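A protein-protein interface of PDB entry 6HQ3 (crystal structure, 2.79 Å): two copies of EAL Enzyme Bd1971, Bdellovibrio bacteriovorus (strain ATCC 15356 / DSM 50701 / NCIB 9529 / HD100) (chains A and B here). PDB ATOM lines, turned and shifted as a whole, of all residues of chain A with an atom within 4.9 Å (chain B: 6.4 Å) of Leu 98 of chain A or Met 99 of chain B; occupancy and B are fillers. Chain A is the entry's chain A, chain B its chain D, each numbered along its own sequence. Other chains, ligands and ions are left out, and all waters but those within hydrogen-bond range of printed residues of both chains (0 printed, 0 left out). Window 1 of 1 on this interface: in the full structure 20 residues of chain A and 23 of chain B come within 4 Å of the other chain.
Of the printed residues of chain B, Leu 97 of chain A touches Ile 52. Leu 98 of chain A touches three residues of chain B. Arg 100 of chain A touches none of the printed residues of chain B. Printed residues of chain A within 4 Å of Ile 52 of chain B: Leu 97 and Val 101. Printed residues of chain A within 4 Å of Ala 91 of chain B: Val 95 (3.8 Å). Leu 98 of chain B touches none of the printed residues of chain A. Met 99 of chain B touches two residues of chain A. Printed residues of chain A within 4 Å of Leu 102 of chain B: Leu 102 (3.6 Å). Of the printed residues of chain A, Leu 103 of chain B touches Leu 102. The nearest residue of chain A that does not touch Met 99 of chain B is Val 95 of chain A (4.6 Å). The nearest printed residue of chain A that does not touch Val 95 of chain B is Met 99 of chain A (4.2 Å).
Of the 9 printed residues of chain A, 6 touch a printed residue of chain B. Hydrophobic or aromatic side chains of chain B within 4 Å of the printed part of chain A: Ile 52, Val 88, Ala 91, Val 95, Met 99, Leu 102 and Leu 103. Among the printed residues, 11 pairs touch across the chains. Among the printed residues, no Asp or Glu carboxylate lies within 4 Å of a Lys or Arg side-chain nitrogen of the other chain.
O of Ala 91 of chain B sits at hydrogen-bond distance from NE2 of Gln 96 of chain B, 2.9 Å away. The backbone carbonyl oxygen (O) of Val 88 of chain B lies within hydrogen-bond range of the side-chain amide nitrogen (NE2) of Gln 96 of chain B (3.2 Å).
Val 95 of chain B touches its own counterpart, Val 95 of chain A. Leu 98 of chain A touches Met 99 of chain B, but with the chains exchanged Met 99 of chain A does not touch Leu 98 of chain B (4.3 Å). Met 99 of chain A touches its own counterpart, Met 99 of chain B. Leu 102 of chain B touches its own counterpart, Leu 102 of chain A.
Ala 91 of chain B touches Val 95 of chain A (CB to CG2, 3.8 Å). Val 95 of chain B touches Val 95 of chain A. O of Leu 97 of chain A touches CG2 of Ile 52 of chain B (3.7 Å). CG2 of Val 88 of chain B touches CD1 of Leu 98 of chain A (3.5 Å). Met 99 of chain B touches Leu 98 of chain A (CE to CD1, 3.8 Å). Met 99 of chain A touches Met 99 of chain B (SD to CG, 3.4 Å). Ile 52 of chain B touches Val 101 of chain A (O to CG2, 3.9 Å). Val 101 of chain A touches Glu 55 of chain B. Leu 102 of chain B touches Leu 102 of chain A. Leu 102 of chain A touches Leu 103 of chain B.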
ATOM      1  N   VAL A  94      21.640 -26.893  17.822  1.00  0.00           N
ATOM      2  CA  VAL A  94      21.380 -25.960  16.729  1.00  0.00           C
ATOM      3  C   VAL A  94      19.883 -25.715  16.561  1.00  0.00           C
ATOM      4  O   VAL A  94      19.474 -24.584  16.297  1.00  0.00           O
ATOM      5  CB  VAL A  94      22.042 -26.431  15.415  1.00  0.00           C
ATOM      6  CG1 VAL A  94      21.536 -25.629  14.225  1.00  0.00           C
ATOM      7  CG2 VAL A  94      23.555 -26.334  15.541  1.00  0.00           C
ATOM      8  N   VAL A  95      19.082 -26.762  16.736  1.00  0.00           N
ATOM      9  CA  VAL A  95      17.629 -26.636  16.636  1.00  0.00           C
ATOM     10  C   VAL A  95      17.121 -25.728  17.759  1.00  0.00           C
ATOM     11  O   VAL A  95      16.341 -24.808  17.505  1.00  0.00           O
ATOM     12  CB  VAL A  95      16.923 -28.028  16.631  1.00  0.00           C
ATOM     13  CG1 VAL A  95      15.419 -27.910  16.875  1.00  0.00           C
ATOM     14  CG2 VAL A  95      17.187 -28.758  15.313  1.00  0.00           C
ATOM     15  N   GLN A  96      17.601 -25.954  18.982  1.00  0.00           N
ATOM     16  CA  GLN A  96      17.240 -25.106  20.120  1.00  0.00           C
ATOM     17  C   GLN A  96      17.563 -23.636  19.838  1.00  0.00           C
ATOM     18  O   GLN A  96      16.713 -22.753  20.050  1.00  0.00           O
ATOM     19  CB  GLN A  96      17.973 -25.513  21.389  1.00  0.00           C
ATOM     20  CG  GLN A  96      17.673 -26.871  21.906  1.00  0.00           C
ATOM     21  CD  GLN A  96      18.192 -27.131  23.290  1.00  0.00           C
ATOM     22  OE1 GLN A  96      18.275 -26.228  24.123  1.00  0.00           O
ATOM     23  NE2 GLN A  96      18.387 -28.413  23.590  1.00  0.00           N
ATOM     24  N   LEU A  97      18.778 -23.387  19.348  1.00  0.00           N
ATOM     25  CA  LEU A  97      19.186 -22.039  18.998  1.00  0.00           C
ATOM     26  C   LEU A  97      18.309 -21.397  17.942  1.00  0.00           C
ATOM     27  O   LEU A  97      17.999 -20.225  18.057  1.00  0.00           O
ATOM     28  CB  LEU A  97      20.629 -22.020  18.505  1.00  0.00           C
ATOM     29  CG  LEU A  97      21.723 -22.186  19.559  1.00  0.00           C
ATOM     30  CD1 LEU A  97      23.074 -22.134  18.879  1.00  0.00           C
ATOM     31  CD2 LEU A  97      21.684 -21.190  20.699  1.00  0.00           C
ATOM     32  N   LEU A  98      17.912 -22.157  16.921  1.00  0.00           N
ATOM     33  CA  LEU A  98      16.996 -21.639  15.903  1.00  0.00           C
ATOM     34  C   LEU A  98      15.644 -21.289  16.475  1.00  0.00           C
ATOM     35  O   LEU A  98      15.128 -20.213  16.180  1.00  0.00           O
ATOM     36  CB  LEU A  98      16.792 -22.635  14.758  1.00  0.00           C
ATOM     37  CG  LEU A  98      17.939 -22.747  13.770  1.00  0.00           C
ATOM     38  CD1 LEU A  98      17.622 -23.797  12.715  1.00  0.00           C
ATOM     39  CD2 LEU A  98      18.193 -21.395  13.127  1.00  0.00           C
ATOM     40  N   MET A  99      15.080 -22.177  17.287  1.00  0.00           N
ATOM     41  CA  MET A  99      13.809 -21.888  17.923  1.00  0.00           C
ATOM     42  C   MET A  99      13.827 -20.604  18.760  1.00  0.00           C
ATOM     43  O   MET A  99      12.862 -19.825  18.716  1.00  0.00           O
ATOM     44  CB  MET A  99      13.331 -23.068  18.765  1.00  0.00           C
ATOM     45  CG  MET A  99      12.709 -24.191  17.947  1.00  0.00           C
ATOM     46  SD  MET A  99      11.020 -23.981  17.335  1.00  0.00           S
ATOM     47  CE  MET A  99      10.211 -23.523  18.869  1.00  0.00           C
ATOM     48  N   ARG A 100      14.927 -20.354  19.466  1.00  0.00           N
ATOM     49  CA  ARG A 100      15.003 -19.162  20.278  1.00  0.00           C
ATOM     50  C   ARG A 100      14.952 -17.895  19.448  1.00  0.00           C
ATOM     51  O   ARG A 100      14.151 -16.997  19.755  1.00  0.00           O
ATOM     52  CB  ARG A 100      16.252 -19.154  21.157  1.00  0.00           C
ATOM     53  CG  ARG A 100      16.262 -20.293  22.148  1.00  0.00           C
ATOM     54  CD  ARG A 100      16.734 -19.937  23.547  1.00  0.00           C
ATOM     55  NE  ARG A 100      17.318 -21.147  24.123  1.00  0.00           N
ATOM     56  CZ  ARG A 100      18.597 -21.537  24.011  1.00  0.00           C
ATOM     57  NH1 ARG A 100      19.489 -20.800  23.338  1.00  0.00           N
ATOM     58  NH2 ARG A 100      18.972 -22.701  24.552  1.00  0.00           N
ATOM     59  N   VAL A 101      15.777 -17.826  18.387  1.00  0.00           N
ATOM     60  CA  VAL A 101      15.866 -16.595  17.595  1.00  0.00           C
ATOM     61  C   VAL A 101      14.645 -16.373  16.723  1.00  0.00           C
ATOM     62  O   VAL A 101      14.289 -15.235  16.438  1.00  0.00           O
ATOM     63  CB  VAL A 101      17.152 -16.508  16.732  1.00  0.00           C
ATOM     64  CG1 VAL A 101      17.012 -17.411  15.528  1.00  0.00           C
ATOM     65  CG2 VAL A 101      17.466 -15.088  16.351  1.00  0.00           C
ATOM     66  N   LEU A 102      14.005 -17.460  16.302  1.00  0.00           N
ATOM     67  CA  LEU A 102      12.723 -17.364  15.624  1.00  0.00           C
ATOM     68  C   LEU A 102      11.690 -16.701  16.535  1.00  0.00           C
ATOM     69  O   LEU A 102      11.061 -15.713  16.128  1.00  0.00           O
ATOM     70  CB  LEU A 102      12.234 -18.753  15.193  1.00  0.00           C
ATOM     71  CG  LEU A 102      12.696 -19.271  13.789  1.00  0.00           C
ATOM     72  CD1 LEU A 102      11.934 -18.468  12.728  1.00  0.00           C
ATOM     73  CD2 LEU A 102      14.207 -19.299  13.465  1.00  0.00           C
ATOM     74  N   ILE B  52      22.437 -17.355  17.479  1.00  0.00           N
ATOM     75  CA  ILE B  52      22.715 -17.780  16.107  1.00  0.00           C
ATOM     76  C   ILE B  52      22.110 -16.819  15.086  1.00  0.00           C
ATOM     77  O   ILE B  52      20.998 -16.306  15.267  1.00  0.00           O
ATOM     78  CB  ILE B  52      22.242 -19.234  15.840  1.00  0.00           C
ATOM     79  CG1 ILE B  52      22.836 -19.775  14.546  1.00  0.00           C
ATOM     80  CG2 ILE B  52      20.728 -19.342  15.783  1.00  0.00           C
ATOM     81  CD1 ILE B  52      22.579 -21.248  14.326  1.00  0.00           C
ATOM     82  N   GLU B  55      20.862 -17.986   9.384  1.00  0.00           N
ATOM     83  CA  GLU B  55      20.116 -19.167   9.032  1.00  0.00           C
ATOM     84  C   GLU B  55      19.247 -18.983   7.765  1.00  0.00           C
ATOM     85  O   GLU B  55      19.011 -19.953   7.077  1.00  0.00           O
ATOM     86  CB  GLU B  55      19.301 -19.669  10.234  1.00  0.00           C
ATOM     87  CG  GLU B  55      18.050 -18.872  10.615  1.00  0.00           C
ATOM     88  CD  GLU B  55      18.309 -17.675  11.500  1.00  0.00           C
ATOM     89  OE1 GLU B  55      19.477 -17.367  11.861  1.00  0.00           O
ATOM     90  OE2 GLU B  55      17.310 -17.046  11.920  1.00  0.00           O
ATOM     91  N   ILE B  59      17.985 -22.013   5.077  1.00  0.00           N
ATOM     92  CA  ILE B  59      16.713 -22.751   5.063  1.00  0.00           C
ATOM     93  C   ILE B  59      15.814 -22.282   3.917  1.00  0.00           C
ATOM     94  O   ILE B  59      15.191 -23.135   3.248  1.00  0.00           O
ATOM     95  CB  ILE B  59      15.946 -22.801   6.418  1.00  0.00           C
ATOM     96  CG1 ILE B  59      15.005 -21.627   6.609  1.00  0.00           C
ATOM     97  CG2 ILE B  59      16.864 -22.967   7.617  1.00  0.00           C
ATOM     98  CD1 ILE B  59      15.676 -20.346   6.821  1.00  0.00           C
ATOM     99  N   VAL B  84      22.943 -27.455   9.202  1.00  0.00           N
ATOM    100  CA  VAL B  84      21.673 -26.833   9.607  1.00  0.00           C
ATOM    101  C   VAL B  84      20.463 -27.610   9.043  1.00  0.00           C
ATOM    102  O   VAL B  84      19.519 -27.958   9.784  1.00  0.00           O
ATOM    103  CB  VAL B  84      21.602 -25.350   9.178  1.00  0.00           C
ATOM    104  CG1 VAL B  84      20.237 -24.740   9.506  1.00  0.00           C
ATOM    105  CG2 VAL B  84      22.712 -24.548   9.824  1.00  0.00           C
ATOM    106  N   VAL B  88      17.878 -29.675  11.316  1.00  0.00           N
ATOM    107  CA  VAL B  88      16.462 -29.331  11.287  1.00  0.00           C
ATOM    108  C   VAL B  88      15.622 -30.512  10.743  1.00  0.00           C
ATOM    109  O   VAL B  88      14.590 -30.868  11.313  1.00  0.00           O
ATOM    110  CB  VAL B  88      16.195 -28.038  10.489  1.00  0.00           C
ATOM    111  CG1 VAL B  88      14.692 -27.745  10.410  1.00  0.00           C
ATOM    112  CG2 VAL B  88      16.920 -26.853  11.115  1.00  0.00           C
ATOM    113  N   ALA B  91      15.156 -33.200  13.323  1.00  0.00           N
ATOM    114  CA  ALA B  91      14.476 -32.756  14.529  1.00  0.00           C
ATOM    115  C   ALA B  91      13.065 -33.325  14.678  1.00  0.00           C
ATOM    116  O   ALA B  91      12.511 -33.902  13.746  1.00  0.00           O
ATOM    117  CB  ALA B  91      14.414 -31.246  14.552  1.00  0.00           C
ATOM    118  N   VAL B  94       6.998 -32.161  15.877  1.00  0.00           N
ATOM    119  CA  VAL B  94       6.283 -31.006  16.397  1.00  0.00           C
ATOM    120  C   VAL B  94       7.146 -29.748  16.358  1.00  0.00           C
ATOM    121  O   VAL B  94       6.652 -28.648  16.063  1.00  0.00           O
ATOM    122  CB  VAL B  94       5.708 -31.268  17.808  1.00  0.00           C
ATOM    123  CG1 VAL B  94       5.191 -29.990  18.429  1.00  0.00           C
ATOM    124  CG2 VAL B  94       4.596 -32.303  17.723  1.00  0.00           C
ATOM    125  N   VAL B  95       8.432 -29.910  16.644  1.00  0.00           N
ATOM    126  CA  VAL B  95       9.375 -28.793  16.606  1.00  0.00           C
ATOM    127  C   VAL B  95       9.481 -28.280  15.159  1.00  0.00           C
ATOM    128  O   VAL B  95       9.390 -27.078  14.914  1.00  0.00           O
ATOM    129  CB  VAL B  95      10.751 -29.185  17.210  1.00  0.00           C
ATOM    130  CG1 VAL B  95      11.848 -28.186  16.848  1.00  0.00           C
ATOM    131  CG2 VAL B  95      10.646 -29.355  18.724  1.00  0.00           C
ATOM    132  N   GLN B  96       9.624 -29.195  14.208  1.00  0.00           N
ATOM    133  CA  GLN B  96       9.649 -28.820  12.785  1.00  0.00           C
ATOM    134  C   GLN B  96       8.408 -28.067  12.374  1.00  0.00           C
ATOM    135  O   GLN B  96       8.508 -27.057  11.724  1.00  0.00           O
ATOM    136  CB  GLN B  96       9.800 -30.048  11.893  1.00  0.00           C
ATOM    137  CG  GLN B  96      11.167 -30.720  12.051  1.00  0.00           C
ATOM    138  CD  GLN B  96      11.506 -31.597  10.861  1.00  0.00           C
ATOM    139  OE1 GLN B  96      11.183 -31.245   9.703  1.00  0.00           O
ATOM    140  NE2 GLN B  96      12.038 -32.773  11.134  1.00  0.00           N
ATOM    141  N   LEU B  97       7.243 -28.566  12.767  1.00  0.00           N
ATOM    142  CA  LEU B  97       5.979 -27.883  12.488  1.00  0.00           C
ATOM    143  C   LEU B  97       5.925 -26.471  13.062  1.00  0.00           C
ATOM    144  O   LEU B  97       5.433 -25.567  12.408  1.00  0.00           O
ATOM    145  CB  LEU B  97       4.803 -28.680  13.020  1.00  0.00           C
ATOM    146  CG  LEU B  97       3.676 -28.847  11.999  1.00  0.00           C
ATOM    147  CD1 LEU B  97       4.131 -29.675  10.805  1.00  0.00           C
ATOM    148  CD2 LEU B  97       2.461 -29.480  12.650  1.00  0.00           C
ATOM    149  N   LEU B  98       6.420 -26.286  14.281  1.00  0.00           N
ATOM    150  CA  LEU B  98       6.485 -24.947  14.865  1.00  0.00           C
ATOM    151  C   LEU B  98       7.414 -24.021  14.098  1.00  0.00           C
ATOM    152  O   LEU B  98       7.068 -22.880  13.807  1.00  0.00           O
ATOM    153  CB  LEU B  98       6.908 -24.995  16.320  1.00  0.00           C
ATOM    154  CG  LEU B  98       5.838 -25.475  17.296  1.00  0.00           C
ATOM    155  CD1 LEU B  98       6.403 -25.506  18.716  1.00  0.00           C
ATOM    156  CD2 LEU B  98       4.618 -24.565  17.235  1.00  0.00           C
ATOM    157  N   MET B  99       8.593 -24.510  13.766  1.00  0.00           N
ATOM    158  CA  MET B  99       9.525 -23.731  12.952  1.00  0.00           C
ATOM    159  C   MET B  99       8.937 -23.305  11.605  1.00  0.00           C
ATOM    160  O   MET B  99       9.175 -22.215  11.148  1.00  0.00           O
ATOM    161  CB  MET B  99      10.838 -24.482  12.770  1.00  0.00           C
ATOM    162  CG  MET B  99      11.748 -24.348  13.990  1.00  0.00           C
ATOM    163  SD  MET B  99      13.352 -25.153  13.853  1.00  0.00           S
ATOM    164  CE  MET B  99      13.930 -24.454  12.302  1.00  0.00           C
ATOM    165  N   ARG B 100       8.154 -24.158  10.973  1.00  0.00           N
ATOM    166  CA  ARG B 100       7.543 -23.802   9.689  1.00  0.00           C
ATOM    167  C   ARG B 100       6.579 -22.645   9.834  1.00  0.00           C
ATOM    168  O   ARG B 100       6.670 -21.708   9.060  1.00  0.00           O
ATOM    169  CB  ARG B 100       6.866 -24.991   9.043  1.00  0.00           C
ATOM    170  CG  ARG B 100       7.907 -26.048   8.662  1.00  0.00           C
ATOM    171  CD  ARG B 100       7.419 -26.979   7.593  1.00  0.00           C
ATOM    172  NE  ARG B 100       6.910 -28.231   8.159  1.00  0.00           N
ATOM    173  CZ  ARG B 100       7.652 -29.289   8.513  1.00  0.00           C
ATOM    174  NH1 ARG B 100       8.990 -29.309   8.360  1.00  0.00           N
ATOM    175  NH2 ARG B 100       7.038 -30.357   9.028  1.00  0.00           N
ATOM    176  N   VAL B 101       5.679 -22.694  10.808  1.00  0.00           N
ATOM    177  CA  VAL B 101       4.663 -21.625  10.966  1.00  0.00           C
ATOM    178  C   VAL B 101       5.256 -20.318  11.490  1.00  0.00           C
ATOM    179  O   VAL B 101       4.766 -19.239  11.185  1.00  0.00           O
ATOM    180  CB  VAL B 101       3.423 -22.026  11.806  1.00  0.00           C
ATOM    181  CG1 VAL B 101       2.637 -23.143  11.125  1.00  0.00           C
ATOM    182  CG2 VAL B 101       3.743 -22.364  13.243  1.00  0.00           C
ATOM    183  N   LEU B 102       6.301 -20.426  12.290  1.00  0.00           N
ATOM    184  CA  LEU B 102       7.084 -19.258  12.664  1.00  0.00           C
ATOM    185  C   LEU B 102       7.658 -18.557  11.426  1.00  0.00           C
ATOM    186  O   LEU B 102       7.464 -17.362  11.231  1.00  0.00           O
ATOM    187  CB  LEU B 102       8.213 -19.653  13.627  1.00  0.00           C
ATOM    188  CG  LEU B 102       7.945 -19.726  15.143  1.00  0.00           C
ATOM    189  CD1 LEU B 102       6.585 -20.253  15.648  1.00  0.00           C
ATOM    190  CD2 LEU B 102       9.099 -20.475  15.810  1.00  0.00           C
ATOM    191  N   LEU B 103       8.354 -19.316  10.590  1.00  0.00           N
ATOM    192  CA  LEU B 103       8.962 -18.782   9.361  1.00  0.00           C
ATOM    193  C   LEU B 103       7.903 -18.235   8.407  1.00  0.00           C
ATOM    194  O   LEU B 103       8.065 -17.153   7.872  1.00  0.00           O
ATOM    195  CB  LEU B 103       9.831 -19.838   8.666  1.00  0.00           C
ATOM    196  CG  LEU B 103      11.085 -20.296   9.448  1.00  0.00           C
ATOM    197  CD1 LEU B 103      11.606 -21.617   8.899  1.00  0.00           C
ATOM    198  CD2 LEU B 103      12.203 -19.257   9.476  1.00  0.00           C
ATOM    199  N   LYS B 104       6.815 -18.965   8.226  1.00  0.00           N
ATOM    200  CA  LYS B 104       5.682 -18.495   7.428  1.00  0.00           C
ATOM    201  C   LYS B 104       5.136 -17.168   7.967  1.00  0.00           C
ATOM    202  O   LYS B 104       4.792 -16.271   7.189  1.00  0.00           O
ATOM    203  CB  LYS B 104       4.579 -19.559   7.367  1.00  0.00           C
ATOM    204  CG  LYS B 104       3.329 -19.171   6.581  1.00  0.00           C
ATOM    205  CD  LYS B 104       2.334 -20.319   6.482  1.00  0.00           C
ATOM    206  CE  LYS B 104       1.610 -20.572   7.807  1.00  0.00           C
ATOM    207  NZ  LYS B 104       0.507 -21.566   7.657  1.00  0.00           N
ATOM    208  N   ARG B 107       7.649 -14.231   7.218  1.00  0.00           N
ATOM    209  CA  ARG B 107       7.548 -13.782   5.836  1.00  0.00           C
ATOM    210  C   ARG B 107       6.362 -12.853   5.593  1.00  0.00           C
ATOM    211  O   ARG B 107       6.514 -11.857   4.893  1.00  0.00           O
ATOM    212  CB  ARG B 107       7.511 -14.975   4.881  1.00  0.00           C
ATOM    213  CG  ARG B 107       8.823 -15.740   4.885  1.00  0.00           C
ATOM    214  CD  ARG B 107       8.898 -16.830   3.830  1.00  0.00           C
ATOM    215  NE  ARG B 107       9.592 -18.014   4.361  1.00  0.00           N
ATOM    216  CZ  ARG B 107       9.018 -19.148   4.793  1.00  0.00           C
ATOM    217  NH1 ARG B 107       7.688 -19.326   4.756  1.00  0.00           N
ATOM    218  NH2 ARG B 107       9.784 -20.138   5.258  1.00  0.00           N
